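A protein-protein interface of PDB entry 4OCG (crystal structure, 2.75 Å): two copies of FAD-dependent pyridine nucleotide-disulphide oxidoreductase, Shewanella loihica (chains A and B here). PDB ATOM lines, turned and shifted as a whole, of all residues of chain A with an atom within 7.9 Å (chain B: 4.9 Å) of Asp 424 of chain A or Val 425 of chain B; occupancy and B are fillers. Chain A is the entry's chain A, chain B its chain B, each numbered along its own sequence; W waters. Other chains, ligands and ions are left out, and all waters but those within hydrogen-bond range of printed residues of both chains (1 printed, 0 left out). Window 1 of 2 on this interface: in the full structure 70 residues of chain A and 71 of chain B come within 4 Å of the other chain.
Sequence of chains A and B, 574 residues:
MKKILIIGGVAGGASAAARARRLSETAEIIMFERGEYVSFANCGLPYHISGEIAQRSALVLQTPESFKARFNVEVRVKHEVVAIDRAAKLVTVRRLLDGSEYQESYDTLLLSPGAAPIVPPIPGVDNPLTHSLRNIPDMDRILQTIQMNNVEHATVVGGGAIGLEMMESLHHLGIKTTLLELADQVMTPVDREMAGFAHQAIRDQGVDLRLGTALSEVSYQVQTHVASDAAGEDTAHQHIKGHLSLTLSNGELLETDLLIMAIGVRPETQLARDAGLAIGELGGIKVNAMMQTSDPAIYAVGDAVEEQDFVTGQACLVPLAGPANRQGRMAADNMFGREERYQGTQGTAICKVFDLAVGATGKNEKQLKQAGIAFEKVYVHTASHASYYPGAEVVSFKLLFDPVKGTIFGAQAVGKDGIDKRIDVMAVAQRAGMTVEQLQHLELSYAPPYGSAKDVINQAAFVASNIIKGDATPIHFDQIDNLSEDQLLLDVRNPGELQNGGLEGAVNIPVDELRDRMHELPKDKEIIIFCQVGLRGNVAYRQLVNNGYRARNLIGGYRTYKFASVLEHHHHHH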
ATOM      1  N   GLN A 346       0.413   2.352   6.973  1.00  0.00           N
ATOM      2  CA  GLN A 346       0.669   2.948   5.695  1.00  0.00           C
ATOM      3  C   GLN A 346       1.125   1.912   4.700  1.00  0.00           C
ATOM      4  O   GLN A 346       1.156   2.167   3.506  1.00  0.00           O
ATOM      5  CB  GLN A 346       1.743   4.008   5.830  1.00  0.00           C
ATOM      6  CG  GLN A 346       1.276   5.260   6.459  1.00  0.00           C
ATOM      7  CD  GLN A 346       2.434   6.001   7.013  1.00  0.00           C
ATOM      8  OE1 GLN A 346       2.886   5.678   8.130  1.00  0.00           O
ATOM      9  NE2 GLN A 346       2.975   6.993   6.240  1.00  0.00           N
ATOM     10  N   THR A 348       4.204   0.786   4.665  1.00  0.00           N
ATOM     11  CA  THR A 348       5.606   1.112   4.367  1.00  0.00           C
ATOM     12  C   THR A 348       6.326  -0.215   4.153  1.00  0.00           C
ATOM     13  O   THR A 348       6.274  -1.045   5.026  1.00  0.00           O
ATOM     14  CB  THR A 348       6.240   1.807   5.594  1.00  0.00           C
ATOM     15  OG1 THR A 348       5.507   2.997   5.937  1.00  0.00           O
ATOM     16  CG2 THR A 348       7.658   2.132   5.309  1.00  0.00           C
ATOM     17  N   ALA A 349       6.971  -0.435   3.020  1.00  0.00           N
ATOM     18  CA  ALA A 349       7.812  -1.648   2.857  1.00  0.00           C
ATOM     19  C   ALA A 349       9.069  -1.359   2.089  1.00  0.00           C
ATOM     20  O   ALA A 349       9.130  -0.359   1.374  1.00  0.00           O
ATOM     21  CB  ALA A 349       7.075  -2.766   2.147  1.00  0.00           C
ATOM     22  N   ILE A 350      10.064  -2.243   2.224  1.00  0.00           N
ATOM     23  CA  ILE A 350      11.247  -2.270   1.354  1.00  0.00           C
ATOM     24  C   ILE A 350      11.796  -3.712   1.158  1.00  0.00           C
ATOM     25  O   ILE A 350      11.668  -4.583   2.020  1.00  0.00           O
ATOM     26  CB  ILE A 350      12.291  -1.353   1.874  1.00  0.00           C
ATOM     27  CG1 ILE A 350      13.274  -1.010   0.768  1.00  0.00           C
ATOM     28  CG2 ILE A 350      12.990  -1.941   3.101  1.00  0.00           C
ATOM     29  CD1 ILE A 350      14.196   0.170   1.137  1.00  0.00           C
ATOM     30  N   ALA A 360       8.209   1.326  -0.771  1.00  0.00           N
ATOM     31  CA  ALA A 360       6.986   2.084  -0.990  1.00  0.00           C
ATOM     32  C   ALA A 360       6.298   2.365   0.297  1.00  0.00           C
ATOM     33  O   ALA A 360       6.528   1.659   1.308  1.00  0.00           O
ATOM     34  CB  ALA A 360       6.025   1.353  -1.878  1.00  0.00           C
ATOM     35  N   THR A 361       5.430   3.375   0.269  1.00  0.00           N
ATOM     36  CA  THR A 361       4.609   3.615   1.407  1.00  0.00           C
ATOM     37  C   THR A 361       3.264   4.093   0.898  1.00  0.00           C
ATOM     38  O   THR A 361       3.169   4.592  -0.233  1.00  0.00           O
ATOM     39  CB  THR A 361       5.305   4.616   2.386  1.00  0.00           C
ATOM     40  OG1 THR A 361       4.783   4.446   3.701  1.00  0.00           O
ATOM     41  CG2 THR A 361       5.150   6.104   1.971  1.00  0.00           C
ATOM     42  N   GLY A 418      20.266   5.006  -1.343  1.00  0.00           N
ATOM     43  CA  GLY A 418      19.466   6.012  -0.626  1.00  0.00           C
ATOM     44  C   GLY A 418      17.950   5.905  -0.767  1.00  0.00           C
ATOM     45  O   GLY A 418      17.243   6.940  -0.698  1.00  0.00           O
ATOM     46  N   ILE A 419      17.447   4.674  -0.955  1.00  0.00           N
ATOM     47  CA  ILE A 419      16.002   4.389  -1.173  1.00  0.00           C
ATOM     48  C   ILE A 419      15.231   4.374   0.149  1.00  0.00           C
ATOM     49  O   ILE A 419      14.137   4.993   0.275  1.00  0.00           O
ATOM     50  CB  ILE A 419      15.773   2.998  -1.965  1.00  0.00           C
ATOM     51  CG1 ILE A 419      16.466   2.997  -3.347  1.00  0.00           C
ATOM     52  CG2 ILE A 419      14.334   2.657  -2.097  1.00  0.00           C
ATOM     53  CD1 ILE A 419      16.464   4.341  -4.050  1.00  0.00           C
ATOM     54  N   ASP A 420      15.797   3.651   1.126  1.00  0.00           N
ATOM     55  CA  ASP A 420      15.256   3.634   2.497  1.00  0.00           C
ATOM     56  C   ASP A 420      15.137   5.045   3.061  1.00  0.00           C
ATOM     57  O   ASP A 420      14.154   5.375   3.660  1.00  0.00           O
ATOM     58  CB  ASP A 420      16.066   2.737   3.435  1.00  0.00           C
ATOM     59  CG  ASP A 420      17.551   3.093   3.481  1.00  0.00           C
ATOM     60  OD1 ASP A 420      18.055   3.624   2.484  1.00  0.00           O
ATOM     61  OD2 ASP A 420      18.234   2.825   4.497  1.00  0.00           O
ATOM     62  N   LYS A 421      16.119   5.897   2.805  1.00  0.00           N
ATOM     63  CA  LYS A 421      16.070   7.269   3.264  1.00  0.00           C
ATOM     64  C   LYS A 421      14.849   7.926   2.670  1.00  0.00           C
ATOM     65  O   LYS A 421      14.076   8.574   3.385  1.00  0.00           O
ATOM     66  CB  LYS A 421      17.357   8.021   2.895  1.00  0.00           C
ATOM     67  CG  LYS A 421      17.345   9.478   3.200  1.00  0.00           C
ATOM     68  CD  LYS A 421      18.728  10.088   3.280  1.00  0.00           C
ATOM     69  CE  LYS A 421      19.258  10.561   1.932  1.00  0.00           C
ATOM     70  NZ  LYS A 421      20.521  11.406   2.082  1.00  0.00           N
ATOM     71  N   ARG A 422      14.622   7.738   1.382  1.00  0.00           N
ATOM     72  CA  ARG A 422      13.543   8.490   0.763  1.00  0.00           C
ATOM     73  C   ARG A 422      12.131   8.021   1.123  1.00  0.00           C
ATOM     74  O   ARG A 422      11.232   8.806   1.149  1.00  0.00           O
ATOM     75  CB  ARG A 422      13.739   8.592  -0.739  1.00  0.00           C
ATOM     76  CG  ARG A 422      14.547   9.801  -1.166  1.00  0.00           C
ATOM     77  CD  ARG A 422      15.979   9.610  -0.899  1.00  0.00           C
ATOM     78  NE  ARG A 422      16.708  10.846  -1.073  1.00  0.00           N
ATOM     79  CZ  ARG A 422      18.010  10.904  -1.325  1.00  0.00           C
ATOM     80  NH1 ARG A 422      18.725   9.784  -1.427  1.00  0.00           N
ATOM     81  NH2 ARG A 422      18.599  12.086  -1.436  1.00  0.00           N
ATOM     82  N   ILE A 423      11.961   6.737   1.430  1.00  0.00           N
ATOM     83  CA  ILE A 423      10.660   6.151   1.735  1.00  0.00           C
ATOM     84  C   ILE A 423      10.330   6.559   3.154  1.00  0.00           C
ATOM     85  O   ILE A 423       9.172   6.786   3.476  1.00  0.00           O
ATOM     86  CB  ILE A 423      10.701   4.574   1.523  1.00  0.00           C
ATOM     87  CG1 ILE A 423      10.872   4.236   0.034  1.00  0.00           C
ATOM     88  CG2 ILE A 423       9.451   3.849   2.059  1.00  0.00           C
ATOM     89  CD1 ILE A 423       9.922   5.072  -0.867  1.00  0.00           C
ATOM     90  N   ASP A 424      11.332   6.656   4.023  1.00  0.00           N
ATOM     91  CA  ASP A 424      11.093   7.150   5.387  1.00  0.00           C
ATOM     92  C   ASP A 424      10.711   8.649   5.441  1.00  0.00           C
ATOM     93  O   ASP A 424       9.705   9.016   6.088  1.00  0.00           O
ATOM     94  CB  ASP A 424      12.303   6.891   6.270  1.00  0.00           C
ATOM     95  CG  ASP A 424      12.560   5.418   6.478  1.00  0.00           C
ATOM     96  OD1 ASP A 424      11.872   4.613   5.796  1.00  0.00           O
ATOM     97  OD2 ASP A 424      13.452   5.078   7.316  1.00  0.00           O
ATOM     98  N   VAL A 425      11.500   9.514   4.779  1.00  0.00           N
ATOM     99  CA  VAL A 425      11.095  10.888   4.677  1.00  0.00           C
ATOM    100  C   VAL A 425       9.588  10.908   4.269  1.00  0.00           C
ATOM    101  O   VAL A 425       8.759  11.681   4.813  1.00  0.00           O
ATOM    102  CB  VAL A 425      11.882  11.622   3.605  1.00  0.00           C
ATOM    103  CG1 VAL A 425      11.368  13.064   3.512  1.00  0.00           C
ATOM    104  CG2 VAL A 425      13.361  11.584   3.876  1.00  0.00           C
ATOM    105  N   MET A 426       9.226  10.070   3.311  1.00  0.00           N
ATOM    106  CA  MET A 426       7.879  10.129   2.851  1.00  0.00           C
ATOM    107  C   MET A 426       6.836   9.581   3.856  1.00  0.00           C
ATOM    108  O   MET A 426       5.795  10.222   4.092  1.00  0.00           O
ATOM    109  CB  MET A 426       7.715   9.525   1.470  1.00  0.00           C
ATOM    110  CG  MET A 426       6.692  10.405   0.757  1.00  0.00           C
ATOM    111  SD  MET A 426       7.461  11.944   0.155  1.00  0.00           S
ATOM    112  CE  MET A 426       8.777  11.049  -0.620  1.00  0.00           C
ATOM    113  N   ALA A 427       7.148   8.472   4.450  1.00  0.00           N
ATOM    114  CA  ALA A 427       6.329   7.895   5.430  1.00  0.00           C
ATOM    115  C   ALA A 427       6.072   8.802   6.565  1.00  0.00           C
ATOM    116  O   ALA A 427       5.050   8.698   7.155  1.00  0.00           O
ATOM    117  CB  ALA A 427       6.953   6.678   5.906  1.00  0.00           C
ATOM    118  N   VAL A 428       6.995   9.673   6.916  1.00  0.00           N
ATOM    119  CA  VAL A 428       6.726  10.563   8.023  1.00  0.00           C
ATOM    120  C   VAL A 428       6.007  11.779   7.545  1.00  0.00           C
ATOM    121  O   VAL A 428       5.165  12.299   8.221  1.00  0.00           O
ATOM    122  CB  VAL A 428       7.955  10.939   8.883  1.00  0.00           C
ATOM    123  CG1 VAL A 428       9.194  10.661   8.241  1.00  0.00           C
ATOM    124  CG2 VAL A 428       7.903  12.327   9.243  1.00  0.00           C
ATOM    125  N   ALA A 429       6.331  12.203   6.345  1.00  0.00           N
ATOM    126  CA  ALA A 429       5.657  13.276   5.679  1.00  0.00           C
ATOM    127  C   ALA A 429       4.206  13.020   5.550  1.00  0.00           C
ATOM    128  O   ALA A 429       3.421  13.884   5.731  1.00  0.00           O
ATOM    129  CB  ALA A 429       6.220  13.429   4.360  1.00  0.00           C
ATOM    130  N   GLN A 430       3.842  11.813   5.195  1.00  0.00           N
ATOM    131  CA  GLN A 430       2.476  11.539   4.947  1.00  0.00           C
ATOM    132  C   GLN A 430       1.759  11.238   6.202  1.00  0.00           C
ATOM    133  O   GLN A 430       0.622  11.511   6.317  1.00  0.00           O
ATOM    134  CB  GLN A 430       2.365  10.387   4.035  1.00  0.00           C
ATOM    135  CG  GLN A 430       1.025   9.851   3.971  1.00  0.00           C
ATOM    136  CD  GLN A 430       1.036   8.508   3.458  1.00  0.00           C
ATOM    137  OE1 GLN A 430       1.556   7.630   4.081  1.00  0.00           O
ATOM    138  NE2 GLN A 430       0.505   8.321   2.302  1.00  0.00           N
ATOM    139  N   ARG A 431       2.426  10.661   7.156  1.00  0.00           N
ATOM    140  CA  ARG A 431       1.786  10.454   8.427  1.00  0.00           C
ATOM    141  C   ARG A 431       1.568  11.800   9.129  1.00  0.00           C
ATOM    142  O   ARG A 431       0.571  12.003   9.845  1.00  0.00           O
ATOM    143  CB  ARG A 431       2.542   9.459   9.321  1.00  0.00           C
ATOM    144  CG  ARG A 431       1.817   9.146  10.635  1.00  0.00           C
ATOM    145  CD  ARG A 431       2.450   7.971  11.375  1.00  0.00           C
ATOM    146  NE  ARG A 431       2.201   6.672  10.724  1.00  0.00           N
ATOM    147  CZ  ARG A 431       1.145   5.869  10.939  1.00  0.00           C
ATOM    148  NH1 ARG A 431       0.167   6.183  11.830  1.00  0.00           N
ATOM    149  NH2 ARG A 431       1.064   4.730  10.250  1.00  0.00           N
ATOM    150  N   LEU A 442      11.011  21.313   2.574  1.00  0.00           N
ATOM    151  CA  LEU A 442      11.830  20.399   3.347  1.00  0.00           C
ATOM    152  C   LEU A 442      13.304  20.805   3.233  1.00  0.00           C
ATOM    153  O   LEU A 442      13.736  21.279   2.188  1.00  0.00           O
ATOM    154  CB  LEU A 442      11.657  18.970   2.834  1.00  0.00           C
ATOM    155  CG  LEU A 442      10.335  18.261   3.139  1.00  0.00           C
ATOM    156  CD1 LEU A 442      10.555  16.776   3.254  1.00  0.00           C
ATOM    157  CD2 LEU A 442       9.821  18.755   4.424  1.00  0.00           C
ATOM    158  N   GLU A 443      14.050  20.601   4.311  1.00  0.00           N
ATOM    159  CA  GLU A 443      15.401  21.056   4.439  1.00  0.00           C
ATOM    160  C   GLU A 443      16.139  19.840   4.985  1.00  0.00           C
ATOM    161  O   GLU A 443      16.135  19.578   6.202  1.00  0.00           O
ATOM    162  CB  GLU A 443      15.425  22.218   5.431  1.00  0.00           C
ATOM    163  CG  GLU A 443      16.774  22.815   5.712  1.00  0.00           C
ATOM    164  CD  GLU A 443      16.746  23.793   6.852  1.00  0.00           C
ATOM    165  OE1 GLU A 443      15.749  24.532   7.000  1.00  0.00           O
ATOM    166  OE2 GLU A 443      17.733  23.858   7.603  1.00  0.00           O
ATOM    167  N   LEU A 444      16.750  19.073   4.080  1.00  0.00           N
ATOM    168  CA  LEU A 444      17.359  17.777   4.462  1.00  0.00           C
ATOM    169  C   LEU A 444      18.893  17.917   4.442  1.00  0.00           C
ATOM    170  O   LEU A 444      19.399  19.046   4.284  1.00  0.00           O
ATOM    171  CB  LEU A 444      16.811  16.632   3.607  1.00  0.00           C
ATOM    172  CG  LEU A 444      15.280  16.738   3.463  1.00  0.00           C
ATOM    173  CD1 LEU A 444      14.714  16.146   2.144  1.00  0.00           C
ATOM    174  CD2 LEU A 444      14.546  16.206   4.656  1.00  0.00           C
ATOM    175  N   SER A 445      19.636  16.844   4.688  1.00  0.00           N
ATOM    176  CA  SER A 445      21.041  17.033   4.971  1.00  0.00           C
ATOM    177  C   SER A 445      21.833  17.001   3.692  1.00  0.00           C
ATOM    178  O   SER A 445      21.857  15.994   2.996  1.00  0.00           O
ATOM    179  CB  SER A 445      21.566  15.948   5.881  1.00  0.00           C
ATOM    180  OG  SER A 445      20.578  15.466   6.742  1.00  0.00           O
ATOM    181  N   ILE A 457      13.311  14.479  -2.992  1.00  0.00           N
ATOM    182  CA  ILE A 457      12.054  14.835  -2.345  1.00  0.00           C
ATOM    183  C   ILE A 457      11.676  16.279  -2.658  1.00  0.00           C
ATOM    184  O   ILE A 457      10.495  16.617  -2.742  1.00  0.00           O
ATOM    185  CB  ILE A 457      12.133  14.652  -0.819  1.00  0.00           C
ATOM    186  CG1 ILE A 457      12.366  13.182  -0.470  1.00  0.00           C
ATOM    187  CG2 ILE A 457      10.866  15.168  -0.155  1.00  0.00           C
ATOM    188  CD1 ILE A 457      11.689  12.215  -1.416  1.00  0.00           C
ATOM    189  N   ASP B 420      22.390  10.339   7.991  1.00  0.00           N
ATOM    190  CA  ASP B 420      21.666  11.198   7.053  1.00  0.00           C
ATOM    191  C   ASP B 420      20.144  10.833   7.017  1.00  0.00           C
ATOM    192  O   ASP B 420      19.274  11.719   7.018  1.00  0.00           O
ATOM    193  CB  ASP B 420      22.360  11.161   5.668  1.00  0.00           C
ATOM    194  CG  ASP B 420      22.345   9.809   5.046  1.00  0.00           C
ATOM    195  OD1 ASP B 420      22.448   8.826   5.768  1.00  0.00           O
ATOM    196  OD2 ASP B 420      22.200   9.702   3.837  1.00  0.00           O
ATOM    197  N   LYS B 421      19.845   9.532   7.042  1.00  0.00           N
ATOM    198  CA  LYS B 421      18.476   9.062   7.064  1.00  0.00           C
ATOM    199  C   LYS B 421      17.739   9.455   8.348  1.00  0.00           C
ATOM    200  O   LYS B 421      16.564   9.853   8.315  1.00  0.00           O
ATOM    201  CB  LYS B 421      18.407   7.538   6.875  1.00  0.00           C
ATOM    202  CG  LYS B 421      17.003   6.942   7.166  1.00  0.00           C
ATOM    203  CD  LYS B 421      16.803   5.578   6.543  1.00  0.00           C
ATOM    204  CE  LYS B 421      17.272   4.462   7.520  1.00  0.00           C
ATOM    205  NZ  LYS B 421      17.226   3.102   6.949  1.00  0.00           N
ATOM    206  N   ARG B 422      18.396   9.317   9.490  1.00  0.00           N
ATOM    207  CA  ARG B 422      17.680   9.605  10.727  1.00  0.00           C
ATOM    208  C   ARG B 422      17.578  11.128  10.940  1.00  0.00           C
ATOM    209  O   ARG B 422      16.733  11.592  11.684  1.00  0.00           O
ATOM    210  CB  ARG B 422      18.348   8.910  11.926  1.00  0.00           C
ATOM    211  CG  ARG B 422      17.842   7.558  12.268  1.00  0.00           C
ATOM    212  CD  ARG B 422      17.896   6.636  11.052  1.00  0.00           C
ATOM    213  NE  ARG B 422      17.636   5.239  11.386  1.00  0.00           N
ATOM    214  CZ  ARG B 422      18.285   4.214  10.863  1.00  0.00           C
ATOM    215  NH1 ARG B 422      19.226   4.377   9.956  1.00  0.00           N
ATOM    216  NH2 ARG B 422      17.970   3.013  11.226  1.00  0.00           N
ATOM    217  N   ILE B 423      18.451  11.898  10.281  1.00  0.00           N
ATOM    218  CA  ILE B 423      18.428  13.359  10.436  1.00  0.00           C
ATOM    219  C   ILE B 423      17.403  13.975   9.514  1.00  0.00           C
ATOM    220  O   ILE B 423      16.671  14.896   9.939  1.00  0.00           O
ATOM    221  CB  ILE B 423      19.819  14.006  10.331  1.00  0.00           C
ATOM    222  CG1 ILE B 423      20.612  13.650  11.578  1.00  0.00           C
ATOM    223  CG2 ILE B 423      19.720  15.519  10.248  1.00  0.00           C
ATOM    224  CD1 ILE B 423      19.956  14.198  12.940  1.00  0.00           C
ATOM    225  N   ASP B 424      17.328  13.436   8.285  1.00  0.00           N
ATOM    226  CA  ASP B 424      16.258  13.790   7.341  1.00  0.00           C
ATOM    227  C   ASP B 424      14.876  13.499   7.935  1.00  0.00           C
ATOM    228  O   ASP B 424      14.048  14.388   7.971  1.00  0.00           O
ATOM    229  CB  ASP B 424      16.447  13.085   6.012  1.00  0.00           C
ATOM    230  CG  ASP B 424      17.637  13.660   5.200  1.00  0.00           C
ATOM    231  OD1 ASP B 424      18.353  14.532   5.741  1.00  0.00           O
ATOM    232  OD2 ASP B 424      17.834  13.251   4.009  1.00  0.00           O
ATOM    233  N   VAL B 425      14.655  12.288   8.445  1.00  0.00           N
ATOM    234  CA  VAL B 425      13.411  11.957   9.139  1.00  0.00           C
ATOM    235  C   VAL B 425      13.008  13.010  10.205  1.00  0.00           C
ATOM    236  O   VAL B 425      11.884  13.515  10.199  1.00  0.00           O
ATOM    237  CB  VAL B 425      13.450  10.474   9.769  1.00  0.00           C
ATOM    238  CG1 VAL B 425      12.328  10.275  10.821  1.00  0.00           C
ATOM    239  CG2 VAL B 425      13.361   9.411   8.705  1.00  0.00           C
ATOM    240  N   MET B 426      13.938  13.323  11.102  1.00  0.00           N
ATOM    241  CA  MET B 426      13.694  14.310  12.147  1.00  0.00           C
ATOM    242  C   MET B 426      13.351  15.666  11.541  1.00  0.00           C
ATOM    243  O   MET B 426      12.489  16.383  12.049  1.00  0.00           O
ATOM    244  CB  MET B 426      14.913  14.434  13.063  1.00  0.00           C
ATOM    245  CG  MET B 426      15.060  13.294  14.058  1.00  0.00           C
ATOM    246  SD  MET B 426      13.487  12.797  14.784  1.00  0.00           S
ATOM    247  CE  MET B 426      13.037  14.287  15.670  1.00  0.00           C
ATOM    248  N   ALA B 427      14.012  16.059  10.491  1.00  0.00           N
ATOM    249  CA  ALA B 427      13.727  17.315   9.871  1.00  0.00           C
ATOM    250  C   ALA B 427      12.321  17.396   9.349  1.00  0.00           C
ATOM    251  O   ALA B 427      11.603  18.298   9.629  1.00  0.00           O
ATOM    252  CB  ALA B 427      14.682  17.542   8.812  1.00  0.00           C
ATOM    253  N   VAL B 428      11.916  16.430   8.583  1.00  0.00           N
ATOM    254  CA  VAL B 428      10.586  16.421   8.082  1.00  0.00           C
ATOM    255  C   VAL B 428       9.612  16.530   9.218  1.00  0.00           C
ATOM    256  O   VAL B 428       8.661  17.256   9.173  1.00  0.00           O
ATOM    257  CB  VAL B 428      10.346  15.154   7.349  1.00  0.00           C
ATOM    258  CG1 VAL B 428       8.966  15.039   6.966  1.00  0.00           C
ATOM    259  CG2 VAL B 428      11.167  15.099   6.194  1.00  0.00           C
ATOM    260  N   ALA B 429       9.880  15.780  10.250  1.00  0.00           N
ATOM    261  CA  ALA B 429       8.979  15.596  11.344  1.00  0.00           C
ATOM    262  C   ALA B 429       8.787  16.822  12.146  1.00  0.00           C
ATOM    263  O   ALA B 429       7.711  17.174  12.490  1.00  0.00           O
ATOM    264  CB  ALA B 429       9.497  14.558  12.189  1.00  0.00           C
ATOM    265  N   LEU B 442       5.561   6.284  14.115  1.00  0.00           N
ATOM    266  CA  LEU B 442       6.191   6.248  12.812  1.00  0.00           C
ATOM    267  C   LEU B 442       6.347   4.814  12.274  1.00  0.00           C
ATOM    268  O   LEU B 442       6.653   3.896  13.003  1.00  0.00           O
ATOM    269  CB  LEU B 442       7.542   6.981  12.851  1.00  0.00           C
ATOM    270  CG  LEU B 442       7.493   8.512  12.829  1.00  0.00           C
ATOM    271  CD1 LEU B 442       8.874   9.138  12.755  1.00  0.00           C
ATOM    272  CD2 LEU B 442       6.689   9.001  11.666  1.00  0.00           C
ATOM    273  N   LEU B 444       8.540   3.148   9.577  1.00  0.00           N
ATOM    274  CA  LEU B 444       9.633   3.347   8.603  1.00  0.00           C
ATOM    275  C   LEU B 444       9.931   2.036   7.892  1.00  0.00           C
ATOM    276  O   LEU B 444       9.217   1.077   8.141  1.00  0.00           O
ATOM    277  CB  LEU B 444      10.850   3.997   9.229  1.00  0.00           C
ATOM    278  CG  LEU B 444      10.332   5.110  10.153  1.00  0.00           C
ATOM    279  CD1 LEU B 444      11.396   5.664  11.099  1.00  0.00           C
ATOM    280  CD2 LEU B 444       9.577   6.219   9.382  1.00  0.00           C
ATOM    281  N   SER B 445      10.891   1.973   6.977  1.00  0.00           N
ATOM    282  CA  SER B 445      10.946   0.817   6.121  1.00  0.00           C
ATOM    283  C   SER B 445      11.852  -0.231   6.685  1.00  0.00           C
ATOM    284  O   SER B 445      13.072  -0.046   6.755  1.00  0.00           O
ATOM    285  CB  SER B 445      11.439   1.167   4.724  1.00  0.00           C
ATOM    286  OG  SER B 445      12.374   2.215   4.774  1.00  0.00           O
ATOM    287  N   ILE B 457      14.639   5.989  15.555  1.00  0.00           N
ATOM    288  CA  ILE B 457      13.645   6.989  15.922  1.00  0.00           C
ATOM    289  C   ILE B 457      12.461   6.535  16.782  1.00  0.00           C
ATOM    290  O   ILE B 457      12.096   7.204  17.770  1.00  0.00           O
ATOM    291  CB  ILE B 457      13.229   7.719  14.673  1.00  0.00           C
ATOM    292  CG1 ILE B 457      14.524   8.302  14.090  1.00  0.00           C
ATOM    293  CG2 ILE B 457      12.244   8.746  15.012  1.00  0.00           C
ATOM    294  CD1 ILE B 457      14.378   9.193  13.026  1.00  0.00           C
HETATM  295  O   HOH W   1       6.398  -0.891   8.482  1.00  0.00           O
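Water W1 lies within hydrogen-bond range of O of Leu 444 of chain B (3.5 Å) and O of Thr 348 of chain A (3.5 Å).
Of chain B, only Lys 421 (3.5 Å), Val 425 (3.7 Å), Leu 444 (3.4 Å) and Ser 445 (2.7 Å) come within 4 Å of Asp 424 of chain A.
Of chain A, only Asp 424 (3.7 Å) comes within 4 Å of Val 425 of chain B.
Of the printed residues of chain A, Asp 420 of chain B touches Lys 421 (3.0 Å) and Ser 445 (3.98 Å).
Ile 457 of chain B touches none of the printed residues of chain A.
The nearest printed residue of chain B that does not touch Asp 424 of chain A is Arg 422 of chain B (5.8 Å).
The nearest printed residue of chain B that does not touch Thr 348 of chain A is Leu 442 of chain B (6.6 Å).
Printed residues of chain A that touch a printed residue of chain B: Thr 348, Ile 350, Asp 420, Lys 421, Asp 424, Val 425, Val 428, Ala 429, Leu 442, Glu 443, Leu 444 and Ser 445.
Hydrophobic or aromatic side chains of chain B within 4 Å of the printed part of chain A: Ile 423, Val 425, Ala 427, Val 428, Leu 442 and Leu 444.
Among the printed residues, 23 pairs touch across the chains.
Among the printed residues, merely in contact across the chains: Leu 444 of chain A with Asp 424 of chain B, Val 425 of chain A with Val 428 of chain B, Thr 348 of chain A with Leu 444 of chain B, Asp 424 of chain A with Leu 444 of chain B, Leu 442 of chain A with Val 428 of chain B, Asp 424 of chain A with Lys 421 of chain B, Ser 445 of chain A with Ile 423 of chain B, Glu 443 of chain A with Ala 427 of chain B, Val 428 of chain A with Leu 442 of chain B, Thr 348 of chain A with Ser 445 of chain B, Asp 424 of chain A with Val 425 of chain B, Val 428 of chain A with Val 428 of chain B, Lys 421 of chain A with Lys 421 of chain B, Asp 420 of chain A with Ser 445 of chain B, Ile 350 of chain A with Ser 445 of chain B, Leu 444 of chain A with Val 428 of chain B, Ala 429 of chain A with Val 428 of chain B and Ser 445 of chain A with Asp 420 of chain B.
Asp 424 of chain A touches Ser 445 of chain B, and with the chains exchanged Ser 445 of chain A touches Asp 424 of chain B.
OG1 of Thr 361 of chain A sits at hydrogen-bond distance from OG1 of Thr 348 of chain A.
The side-chain amino group (NZ) of Lys 421 of chain B is in salt-bridge range of the side-chain carboxylate (OD2) of Asp 420 of chain A, 2.7 Å away.
NZ of Lys 421 of chain A is in salt-bridge range of OD2 of Asp 420 of chain B (3.0 Å).
The side-chain amino group (NZ) of Lys 421 of chain A lies within salt-bridge range of the side-chain carboxylate (OD2) of Asp 424 of chain B (3.8 Å).
OD1 of Asp 424 of chain A lies within hydrogen-bond range of OG of Ser 445 of chain B (2.7 Å).
OD1 of Asp 424 of chain B sits at hydrogen-bond distance from OG of Ser 445 of chain A.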
